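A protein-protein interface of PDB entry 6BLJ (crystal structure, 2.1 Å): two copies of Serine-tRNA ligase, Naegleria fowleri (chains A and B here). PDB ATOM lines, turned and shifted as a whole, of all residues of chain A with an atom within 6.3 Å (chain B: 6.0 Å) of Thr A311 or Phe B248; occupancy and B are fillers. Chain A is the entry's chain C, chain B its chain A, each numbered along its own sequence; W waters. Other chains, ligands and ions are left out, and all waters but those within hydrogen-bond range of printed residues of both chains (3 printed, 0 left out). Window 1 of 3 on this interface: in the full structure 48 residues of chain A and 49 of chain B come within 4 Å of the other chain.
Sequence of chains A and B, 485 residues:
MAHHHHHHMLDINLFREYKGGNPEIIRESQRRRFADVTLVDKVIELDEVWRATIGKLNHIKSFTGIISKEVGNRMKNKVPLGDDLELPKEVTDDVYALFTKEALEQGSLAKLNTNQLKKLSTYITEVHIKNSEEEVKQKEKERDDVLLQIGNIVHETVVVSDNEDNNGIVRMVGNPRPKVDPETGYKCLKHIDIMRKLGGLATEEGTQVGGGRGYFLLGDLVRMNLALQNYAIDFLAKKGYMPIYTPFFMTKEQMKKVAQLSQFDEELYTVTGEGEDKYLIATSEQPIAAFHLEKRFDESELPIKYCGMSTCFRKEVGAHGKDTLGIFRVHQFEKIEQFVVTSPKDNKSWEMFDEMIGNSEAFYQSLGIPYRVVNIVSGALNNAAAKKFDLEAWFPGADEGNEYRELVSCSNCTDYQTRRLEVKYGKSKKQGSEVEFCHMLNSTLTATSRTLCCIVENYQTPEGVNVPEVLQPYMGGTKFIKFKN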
ATOM      1  N   TYR A 245     -22.184  38.867 -22.357  1.00  0.00           N
ATOM      2  CA  TYR A 245     -21.573  37.682 -22.939  1.00  0.00           C
ATOM      3  C   TYR A 245     -20.768  38.146 -24.150  1.00  0.00           C
ATOM      4  O   TYR A 245     -21.281  38.921 -24.962  1.00  0.00           O
ATOM      5  CB  TYR A 245     -22.674  36.680 -23.335  1.00  0.00           C
ATOM      6  CG  TYR A 245     -22.236  35.498 -24.200  1.00  0.00           C
ATOM      7  CD1 TYR A 245     -21.849  34.288 -23.627  1.00  0.00           C
ATOM      8  CD2 TYR A 245     -22.248  35.592 -25.590  1.00  0.00           C
ATOM      9  CE1 TYR A 245     -21.464  33.202 -24.419  1.00  0.00           C
ATOM     10  CE2 TYR A 245     -21.853  34.522 -26.387  1.00  0.00           C
ATOM     11  CZ  TYR A 245     -21.457  33.341 -25.803  1.00  0.00           C
ATOM     12  OH  TYR A 245     -21.085  32.289 -26.604  1.00  0.00           O
ATOM     13  N   THR A 246     -19.517  37.696 -24.264  1.00  0.00           N
ATOM     14  CA  THR A 246     -18.584  38.307 -25.213  1.00  0.00           C
ATOM     15  C   THR A 246     -18.186  37.362 -26.348  1.00  0.00           C
ATOM     16  O   THR A 246     -18.339  36.139 -26.240  1.00  0.00           O
ATOM     17  CB  THR A 246     -17.303  38.736 -24.490  1.00  0.00           C
ATOM     18  OG1 THR A 246     -16.545  37.557 -24.175  1.00  0.00           O
ATOM     19  CG2 THR A 246     -17.642  39.487 -23.189  1.00  0.00           C
ATOM     20  N   PHE A 248     -15.534  35.064 -27.947  1.00  0.00           N
ATOM     21  CA  PHE A 248     -14.383  34.375 -27.385  1.00  0.00           C
ATOM     22  C   PHE A 248     -13.142  34.516 -28.278  1.00  0.00           C
ATOM     23  O   PHE A 248     -12.076  34.036 -27.891  1.00  0.00           O
ATOM     24  CB  PHE A 248     -14.683  32.871 -27.148  1.00  0.00           C
ATOM     25  CG  PHE A 248     -15.872  32.580 -26.206  1.00  0.00           C
ATOM     26  CD1 PHE A 248     -16.539  33.600 -25.519  1.00  0.00           C
ATOM     27  CD2 PHE A 248     -16.295  31.268 -26.007  1.00  0.00           C
ATOM     28  CE1 PHE A 248     -17.663  33.308 -24.686  1.00  0.00           C
ATOM     29  CE2 PHE A 248     -17.400  30.962 -25.175  1.00  0.00           C
ATOM     30  CZ  PHE A 248     -18.079  31.993 -24.519  1.00  0.00           C
ATOM     31  N   ILE A 281      -9.677  34.464 -26.309  1.00  0.00           N
ATOM     32  CA  ILE A 281      -9.514  35.338 -25.151  1.00  0.00           C
ATOM     33  C   ILE A 281      -9.071  34.530 -23.941  1.00  0.00           C
ATOM     34  O   ILE A 281      -9.459  33.366 -23.756  1.00  0.00           O
ATOM     35  CB  ILE A 281     -10.810  36.115 -24.842  1.00  0.00           C
ATOM     36  CG1 ILE A 281     -11.913  35.156 -24.372  1.00  0.00           C
ATOM     37  CG2 ILE A 281     -11.219  36.926 -26.085  1.00  0.00           C
ATOM     38  CD1 ILE A 281     -13.214  35.853 -23.892  1.00  0.00           C
ATOM     39  N   ALA A 282      -8.242  35.159 -23.104  1.00  0.00           N
ATOM     40  CA  ALA A 282      -7.841  34.596 -21.819  1.00  0.00           C
ATOM     41  C   ALA A 282      -8.792  34.962 -20.687  1.00  0.00           C
ATOM     42  O   ALA A 282      -8.681  34.385 -19.607  1.00  0.00           O
ATOM     43  CB  ALA A 282      -6.425  35.076 -21.449  1.00  0.00           C
ATOM     44  N   THR A 283      -9.677  35.937 -20.900  1.00  0.00           N
ATOM     45  CA  THR A 283     -10.570  36.490 -19.885  1.00  0.00           C
ATOM     46  C   THR A 283     -11.516  37.449 -20.593  1.00  0.00           C
ATOM     47  O   THR A 283     -11.127  38.095 -21.577  1.00  0.00           O
ATOM     48  CB  THR A 283      -9.798  37.215 -18.759  1.00  0.00           C
ATOM     49  OG1 THR A 283     -10.707  38.002 -17.981  1.00  0.00           O
ATOM     50  CG2 THR A 283      -8.714  38.153 -19.340  1.00  0.00           C
ATOM     51  N   SER A 284     -12.769  37.506 -20.114  1.00  0.00           N
ATOM     52  CA  SER A 284     -13.742  38.416 -20.721  1.00  0.00           C
ATOM     53  C   SER A 284     -13.345  39.873 -20.540  1.00  0.00           C
ATOM     54  O   SER A 284     -13.880  40.737 -21.237  1.00  0.00           O
ATOM     55  CB  SER A 284     -15.154  38.180 -20.169  1.00  0.00           C
ATOM     56  OG  SER A 284     -15.199  38.370 -18.756  1.00  0.00           O
ATOM     57  N   MET A 309     -19.190  37.401 -18.799  1.00  0.00           N
ATOM     58  CA  MET A 309     -19.340  35.954 -18.832  1.00  0.00           C
ATOM     59  C   MET A 309     -18.677  35.405 -20.087  1.00  0.00           C
ATOM     60  O   MET A 309     -18.960  35.876 -21.194  1.00  0.00           O
ATOM     61  CB  MET A 309     -20.830  35.581 -18.808  1.00  0.00           C
ATOM     62  CG  MET A 309     -21.136  34.126 -19.002  1.00  0.00           C
ATOM     63  SD  MET A 309     -22.925  33.825 -19.133  1.00  0.00           S
ATOM     64  CE  MET A 309     -22.827  32.034 -19.179  1.00  0.00           C
ATOM     65  N   SER A 310     -17.818  34.402 -19.924  1.00  0.00           N
ATOM     66  CA  SER A 310     -17.221  33.766 -21.094  1.00  0.00           C
ATOM     67  C   SER A 310     -16.521  32.483 -20.664  1.00  0.00           C
ATOM     68  O   SER A 310     -16.264  32.261 -19.480  1.00  0.00           O
ATOM     69  CB  SER A 310     -16.224  34.707 -21.803  1.00  0.00           C
ATOM     70  OG  SER A 310     -15.002  34.826 -21.071  1.00  0.00           O
ATOM     71  N   THR A 311     -16.252  31.623 -21.641  1.00  0.00           N
ATOM     72  CA  THR A 311     -15.174  30.655 -21.489  1.00  0.00           C
ATOM     73  C   THR A 311     -13.840  31.358 -21.727  1.00  0.00           C
ATOM     74  O   THR A 311     -13.762  32.348 -22.461  1.00  0.00           O
ATOM     75  CB  THR A 311     -15.377  29.479 -22.447  1.00  0.00           C
ATOM     76  OG1 THR A 311     -16.626  28.850 -22.123  1.00  0.00           O
ATOM     77  CG2 THR A 311     -14.256  28.420 -22.296  1.00  0.00           C
ATOM     78  N   CYS A 312     -12.799  30.871 -21.064  1.00  0.00           N
ATOM     79  CA  CYS A 312     -11.460  31.450 -21.121  1.00  0.00           C
ATOM     80  C   CYS A 312     -10.463  30.381 -21.532  1.00  0.00           C
ATOM     81  O   CYS A 312     -10.556  29.234 -21.079  1.00  0.00           O
ATOM     82  CB  CYS A 312     -11.043  32.022 -19.744  1.00  0.00           C
ATOM     83  SG  CYS A 312     -12.214  33.247 -19.097  1.00  0.00           S
ATOM     84  N   PHE A 313      -9.478  30.774 -22.333  1.00  0.00           N
ATOM     85  CA  PHE A 313      -8.502  29.855 -22.911  1.00  0.00           C
ATOM     86  C   PHE A 313      -7.092  30.351 -22.627  1.00  0.00           C
ATOM     87  O   PHE A 313      -6.770  31.511 -22.911  1.00  0.00           O
ATOM     88  CB  PHE A 313      -8.725  29.734 -24.419  1.00  0.00           C
ATOM     89  CG  PHE A 313     -10.124  29.340 -24.790  1.00  0.00           C
ATOM     90  CD1 PHE A 313     -10.449  28.012 -25.026  1.00  0.00           C
ATOM     91  CD2 PHE A 313     -11.121  30.304 -24.906  1.00  0.00           C
ATOM     92  CE1 PHE A 313     -11.756  27.649 -25.392  1.00  0.00           C
ATOM     93  CE2 PHE A 313     -12.415  29.944 -25.275  1.00  0.00           C
ATOM     94  CZ  PHE A 313     -12.721  28.619 -25.512  1.00  0.00           C
ATOM     95  N   GLN A 332      -8.948  25.639 -20.401  1.00  0.00           N
ATOM     96  CA  GLN A 332     -10.299  26.023 -20.776  1.00  0.00           C
ATOM     97  C   GLN A 332     -11.166  26.026 -19.525  1.00  0.00           C
ATOM     98  O   GLN A 332     -11.271  24.997 -18.855  1.00  0.00           O
ATOM     99  CB  GLN A 332     -10.849  25.047 -21.815  1.00  0.00           C
ATOM    100  CG  GLN A 332     -12.310  25.240 -22.179  1.00  0.00           C
ATOM    101  CD  GLN A 332     -12.849  24.043 -22.956  1.00  0.00           C
ATOM    102  OE1 GLN A 332     -12.201  23.563 -23.881  1.00  0.00           O
ATOM    103  NE2 GLN A 332     -14.026  23.545 -22.563  1.00  0.00           N
ATOM    104  N   PHE A 333     -11.777  27.168 -19.211  1.00  0.00           N
ATOM    105  CA  PHE A 333     -12.648  27.280 -18.040  1.00  0.00           C
ATOM    106  C   PHE A 333     -13.592  28.469 -18.220  1.00  0.00           C
ATOM    107  O   PHE A 333     -13.293  29.417 -18.958  1.00  0.00           O
ATOM    108  CB  PHE A 333     -11.827  27.420 -16.735  1.00  0.00           C
ATOM    109  CG  PHE A 333     -10.914  28.652 -16.688  1.00  0.00           C
ATOM    110  CD1 PHE A 333      -9.648  28.614 -17.256  1.00  0.00           C
ATOM    111  CD2 PHE A 333     -11.327  29.829 -16.058  1.00  0.00           C
ATOM    112  CE1 PHE A 333      -8.803  29.732 -17.224  1.00  0.00           C
ATOM    113  CE2 PHE A 333     -10.497  30.968 -16.010  1.00  0.00           C
ATOM    114  CZ  PHE A 333      -9.214  30.912 -16.595  1.00  0.00           C
ATOM    115  N   GLU A 334     -14.743  28.411 -17.544  1.00  0.00           N
ATOM    116  CA  GLU A 334     -15.672  29.541 -17.541  1.00  0.00           C
ATOM    117  C   GLU A 334     -15.371  30.456 -16.363  1.00  0.00           C
ATOM    118  O   GLU A 334     -14.950  29.998 -15.296  1.00  0.00           O
ATOM    119  CB  GLU A 334     -17.132  29.080 -17.460  1.00  0.00           C
ATOM    120  CG  GLU A 334     -17.672  28.501 -18.754  1.00  0.00           C
ATOM    121  CD  GLU A 334     -17.069  27.122 -19.059  1.00  0.00           C
ATOM    122  OE1 GLU A 334     -17.148  26.231 -18.190  1.00  0.00           O
ATOM    123  OE2 GLU A 334     -16.495  26.944 -20.153  1.00  0.00           O
ATOM    124  N   LYS A 335     -15.587  31.762 -16.567  1.00  0.00           N
ATOM    125  CA  LYS A 335     -15.279  32.757 -15.547  1.00  0.00           C
ATOM    126  C   LYS A 335     -16.309  33.866 -15.595  1.00  0.00           C
ATOM    127  O   LYS A 335     -16.648  34.345 -16.677  1.00  0.00           O
ATOM    128  CB  LYS A 335     -13.863  33.341 -15.726  1.00  0.00           C
ATOM    129  CG  LYS A 335     -13.509  34.394 -14.660  1.00  0.00           C
ATOM    130  CD  LYS A 335     -11.998  34.707 -14.598  1.00  0.00           C
ATOM    131  CE  LYS A 335     -11.470  35.246 -15.905  1.00  0.00           C
ATOM    132  NZ  LYS A 335     -12.258  36.426 -16.382  1.00  0.00           N
ATOM    133  N   TYR B 245     -19.828  17.893 -20.014  1.00  0.00           N
ATOM    134  CA  TYR B 245     -19.169  19.090 -20.525  1.00  0.00           C
ATOM    135  C   TYR B 245     -17.846  18.653 -21.158  1.00  0.00           C
ATOM    136  O   TYR B 245     -17.123  17.848 -20.571  1.00  0.00           O
ATOM    137  CB  TYR B 245     -18.938  20.074 -19.370  1.00  0.00           C
ATOM    138  CG  TYR B 245     -18.065  21.271 -19.661  1.00  0.00           C
ATOM    139  CD1 TYR B 245     -18.620  22.491 -20.076  1.00  0.00           C
ATOM    140  CD2 TYR B 245     -16.687  21.201 -19.491  1.00  0.00           C
ATOM    141  CE1 TYR B 245     -17.808  23.604 -20.336  1.00  0.00           C
ATOM    142  CE2 TYR B 245     -15.863  22.297 -19.764  1.00  0.00           C
ATOM    143  CZ  TYR B 245     -16.424  23.498 -20.175  1.00  0.00           C
ATOM    144  OH  TYR B 245     -15.592  24.580 -20.407  1.00  0.00           O
ATOM    145  N   THR B 246     -17.553  19.148 -22.355  1.00  0.00           N
ATOM    146  CA  THR B 246     -16.487  18.605 -23.188  1.00  0.00           C
ATOM    147  C   THR B 246     -15.325  19.581 -23.387  1.00  0.00           C
ATOM    148  O   THR B 246     -15.471  20.789 -23.179  1.00  0.00           O
ATOM    149  CB  THR B 246     -17.046  18.234 -24.572  1.00  0.00           C
ATOM    150  OG1 THR B 246     -17.335  19.433 -25.322  1.00  0.00           O
ATOM    151  CG2 THR B 246     -18.336  17.439 -24.438  1.00  0.00           C
ATOM    152  N   PRO B 247     -14.150  19.085 -23.798  1.00  0.00           N
ATOM    153  CA  PRO B 247     -13.166  19.975 -24.419  1.00  0.00           C
ATOM    154  C   PRO B 247     -13.808  20.683 -25.592  1.00  0.00           C
ATOM    155  O   PRO B 247     -14.632  20.110 -26.306  1.00  0.00           O
ATOM    156  CB  PRO B 247     -12.051  19.022 -24.889  1.00  0.00           C
ATOM    157  CG  PRO B 247     -12.192  17.786 -23.989  1.00  0.00           C
ATOM    158  CD  PRO B 247     -13.692  17.673 -23.782  1.00  0.00           C
ATOM    159  N   PHE B 248     -13.442  21.946 -25.775  1.00  0.00           N
ATOM    160  CA  PHE B 248     -13.828  22.678 -26.971  1.00  0.00           C
ATOM    161  C   PHE B 248     -12.754  22.589 -28.055  1.00  0.00           C
ATOM    162  O   PHE B 248     -12.978  23.114 -29.152  1.00  0.00           O
ATOM    163  CB  PHE B 248     -14.105  24.172 -26.638  1.00  0.00           C
ATOM    164  CG  PHE B 248     -15.218  24.416 -25.606  1.00  0.00           C
ATOM    165  CD1 PHE B 248     -16.010  23.383 -25.120  1.00  0.00           C
ATOM    166  CD2 PHE B 248     -15.468  25.708 -25.142  1.00  0.00           C
ATOM    167  CE1 PHE B 248     -17.015  23.626 -24.156  1.00  0.00           C
ATOM    168  CE2 PHE B 248     -16.481  25.962 -24.189  1.00  0.00           C
ATOM    169  CZ  PHE B 248     -17.253  24.919 -23.702  1.00  0.00           C
ATOM    170  N   PHE B 249     -11.599  21.975 -27.740  1.00  0.00           N
ATOM    171  CA  PHE B 249     -10.486  21.628 -28.630  1.00  0.00           C
ATOM    172  C   PHE B 249     -10.483  20.137 -28.912  1.00  0.00           C
ATOM    173  O   PHE B 249     -10.689  19.345 -27.995  1.00  0.00           O
ATOM    174  CB  PHE B 249      -9.086  21.788 -27.990  1.00  0.00           C
ATOM    175  CG  PHE B 249      -8.738  23.121 -27.489  1.00  0.00           C
ATOM    176  CD1 PHE B 249      -9.239  24.260 -28.064  1.00  0.00           C
ATOM    177  CD2 PHE B 249      -7.836  23.226 -26.435  1.00  0.00           C
ATOM    178  CE1 PHE B 249      -8.860  25.498 -27.586  1.00  0.00           C
ATOM    179  CE2 PHE B 249      -7.457  24.447 -25.955  1.00  0.00           C
ATOM    180  CZ  PHE B 249      -7.974  25.591 -26.524  1.00  0.00           C
ATOM    181  N   MET B 250     -10.056  19.749 -30.111  1.00  0.00           N
ATOM    182  CA  MET B 250      -9.722  18.348 -30.359  1.00  0.00           C
ATOM    183  C   MET B 250      -8.446  18.278 -31.183  1.00  0.00           C
ATOM    184  O   MET B 250      -8.236  19.110 -32.070  1.00  0.00           O
ATOM    185  CB  MET B 250     -10.861  17.624 -31.087  1.00  0.00           C
ATOM    186  CG  MET B 250     -12.062  17.329 -30.217  1.00  0.00           C
ATOM    187  SD  MET B 250     -13.358  16.507 -31.163  1.00  0.00           S
ATOM    188  CE  MET B 250     -12.628  14.893 -31.478  1.00  0.00           C
ATOM    189  N   TYR B 279      -8.350  21.567 -33.517  1.00  0.00           N
ATOM    190  CA  TYR B 279      -9.515  22.205 -34.109  1.00  0.00           C
ATOM    191  C   TYR B 279     -10.471  22.612 -32.997  1.00  0.00           C
ATOM    192  O   TYR B 279     -10.663  21.857 -32.047  1.00  0.00           O
ATOM    193  CB  TYR B 279     -10.294  21.280 -35.065  1.00  0.00           C
ATOM    194  CG  TYR B 279      -9.627  20.904 -36.371  1.00  0.00           C
ATOM    195  CD1 TYR B 279      -9.432  21.848 -37.369  1.00  0.00           C
ATOM    196  CD2 TYR B 279      -9.289  19.582 -36.646  1.00  0.00           C
ATOM    197  CE1 TYR B 279      -8.857  21.502 -38.585  1.00  0.00           C
ATOM    198  CE2 TYR B 279      -8.722  19.223 -37.864  1.00  0.00           C
ATOM    199  CZ  TYR B 279      -8.506  20.185 -38.821  1.00  0.00           C
ATOM    200  OH  TYR B 279      -7.930  19.833 -40.016  1.00  0.00           O
ATOM    201  N   LEU B 280     -11.122  23.768 -33.148  1.00  0.00           N
ATOM    202  CA  LEU B 280     -12.272  24.073 -32.302  1.00  0.00           C
ATOM    203  C   LEU B 280     -13.441  23.193 -32.734  1.00  0.00           C
ATOM    204  O   LEU B 280     -13.667  22.976 -33.928  1.00  0.00           O
ATOM    205  CB  LEU B 280     -12.666  25.547 -32.423  1.00  0.00           C
ATOM    206  CG  LEU B 280     -11.671  26.588 -31.892  1.00  0.00           C
ATOM    207  CD1 LEU B 280     -12.141  27.998 -32.195  1.00  0.00           C
ATOM    208  CD2 LEU B 280     -11.464  26.414 -30.381  1.00  0.00           C
ATOM    209  N   ILE B 281     -14.191  22.680 -31.766  1.00  0.00           N
ATOM    210  CA  ILE B 281     -15.295  21.789 -32.116  1.00  0.00           C
ATOM    211  C   ILE B 281     -16.460  22.575 -32.706  1.00  0.00           C
ATOM    212  O   ILE B 281     -16.733  23.724 -32.317  1.00  0.00           O
ATOM    213  CB  ILE B 281     -15.733  20.968 -30.895  1.00  0.00           C
ATOM    214  CG1 ILE B 281     -16.372  21.859 -29.818  1.00  0.00           C
ATOM    215  CG2 ILE B 281     -14.524  20.171 -30.373  1.00  0.00           C
ATOM    216  CD1 ILE B 281     -16.975  21.026 -28.594  1.00  0.00           C
ATOM    217  N   MET B 309     -22.911  19.393 -23.524  1.00  0.00           N
ATOM    218  CA  MET B 309     -22.961  20.835 -23.343  1.00  0.00           C
ATOM    219  C   MET B 309     -21.646  21.427 -23.818  1.00  0.00           C
ATOM    220  O   MET B 309     -20.584  20.994 -23.360  1.00  0.00           O
ATOM    221  CB  MET B 309     -23.180  21.149 -21.858  1.00  0.00           C
ATOM    222  CG  MET B 309     -23.070  22.594 -21.462  1.00  0.00           C
ATOM    223  SD  MET B 309     -23.080  22.687 -19.652  1.00  0.00           S
ATOM    224  CE  MET B 309     -23.091  24.479 -19.474  1.00  0.00           C
ATOM    225  N   SER B 310     -21.703  22.435 -24.688  1.00  0.00           N
ATOM    226  CA  SER B 310     -20.454  23.075 -25.093  1.00  0.00           C
ATOM    227  C   SER B 310     -20.769  24.364 -25.829  1.00  0.00           C
ATOM    228  O   SER B 310     -21.878  24.557 -26.329  1.00  0.00           O
ATOM    229  CB  SER B 310     -19.602  22.171 -26.008  1.00  0.00           C
ATOM    230  OG  SER B 310     -20.146  22.129 -27.337  1.00  0.00           O
ATOM    231  N   THR B 311     -19.770  25.243 -25.902  1.00  0.00           N
ATOM    232  CA  THR B 311     -19.775  26.220 -26.975  1.00  0.00           C
ATOM    233  C   THR B 311     -19.324  25.508 -28.243  1.00  0.00           C
ATOM    234  O   THR B 311     -18.578  24.526 -28.186  1.00  0.00           O
ATOM    235  CB  THR B 311     -18.880  27.415 -26.618  1.00  0.00           C
ATOM    236  OG1 THR B 311     -19.418  28.031 -25.449  1.00  0.00           O
ATOM    237  CG2 THR B 311     -18.848  28.479 -27.747  1.00  0.00           C
ATOM    238  N   PHE B 313     -18.142  26.189 -32.488  1.00  0.00           N
ATOM    239  CA  PHE B 313     -17.483  27.164 -33.352  1.00  0.00           C
ATOM    240  C   PHE B 313     -17.558  26.703 -34.799  1.00  0.00           C
ATOM    241  O   PHE B 313     -17.191  25.562 -35.110  1.00  0.00           O
ATOM    242  CB  PHE B 313     -16.023  27.366 -32.948  1.00  0.00           C
ATOM    243  CG  PHE B 313     -15.832  27.756 -31.493  1.00  0.00           C
ATOM    244  CD1 PHE B 313     -15.732  29.093 -31.120  1.00  0.00           C
ATOM    245  CD2 PHE B 313     -15.743  26.782 -30.504  1.00  0.00           C
ATOM    246  CE1 PHE B 313     -15.532  29.449 -29.776  1.00  0.00           C
ATOM    247  CE2 PHE B 313     -15.557  27.131 -29.161  1.00  0.00           C
ATOM    248  CZ  PHE B 313     -15.448  28.459 -28.805  1.00  0.00           C
HETATM  249  O   HOH W   1     -15.525  24.355 -17.038  1.00  0.00           O
HETATM  250  O   HOH W   2     -13.136  20.801 -20.898  1.00  0.00           O
HETATM  251  O   HOH W   3     -19.099  28.400 -22.821  1.00  0.00           O
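Of the printed residues of chain B, Phe A248 touches Thr B311. Thr A311 touches just one residue of chain B: Phe B248 (3.6 Å). Printed residues of chain A within 4 Å of Phe B248: Thr A311 and Gln A332. Of the printed residues of chain A, Phe B249 touches Phe A313. Ile B281 touches none of the printed residues of chain A. Ser B310 touches none of the printed residues of chain A.
NE2 of Gln A332 is in hydrogen-bond range of O of Thr B246. OH of Tyr B245 is in hydrogen-bond range of NE2 of Gln A332, at 2.9 Å. OE1 of Gln A332 lies within hydrogen-bond range of N of Phe B248. OH of Tyr B245 is in hydrogen-bond range of OE2 of Glu A334 (2.5 Å).
Water W3 bridges the side-chain hydroxyl of Thr A311 (2.6 Å) and the side-chain hydroxyl of Thr B311 (2.7 Å). Water W1 bridges OE1 of Glu A334 (2.7 Å) and OH of Tyr B245 (3.4 Å). Water W2 lies within hydrogen-bond range of the backbone carbonyl oxygen of Thr B246 (3.3 Å) and the side-chain amide nitrogen of Gln A332 (3.3 Å).
Among the printed residues, pairs that only touch across the chains: Thr A311 with Phe B248, Phe A248 with Thr B311, Gln A332 with Pro B247 and Phe A313 with Phe B249.
Phe A248 touches Thr B311, and with the chains exchanged Thr A311 touches Phe B248. 8 positions are printed for both chains.
Of the 16 printed residues of chain A, 5 touch a printed residue of chain B. Hydrophobic or aromatic side chains of chain A within 4 Å of the printed part of chain B: Phe A248 and Phe A313. Of the 13 printed residues of chain B, 6 touch a printed residue of chain A. Among the printed residues, 8 pairs touch across the chains.
N of Ile A281 sits at hydrogen-bond distance from O of Phe A248. O of Ile A281 is in hydrogen-bond range of N of Phe A313 (3.0 Å). The backbone carbonyl oxygen (O) of Phe B248 lies within hydrogen-bond range of the backbone NH (N) of Ile B281 (2.9 Å). OE2 of Glu A334 sits at hydrogen-bond distance from OG1 of Thr A311 (2.7 Å).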
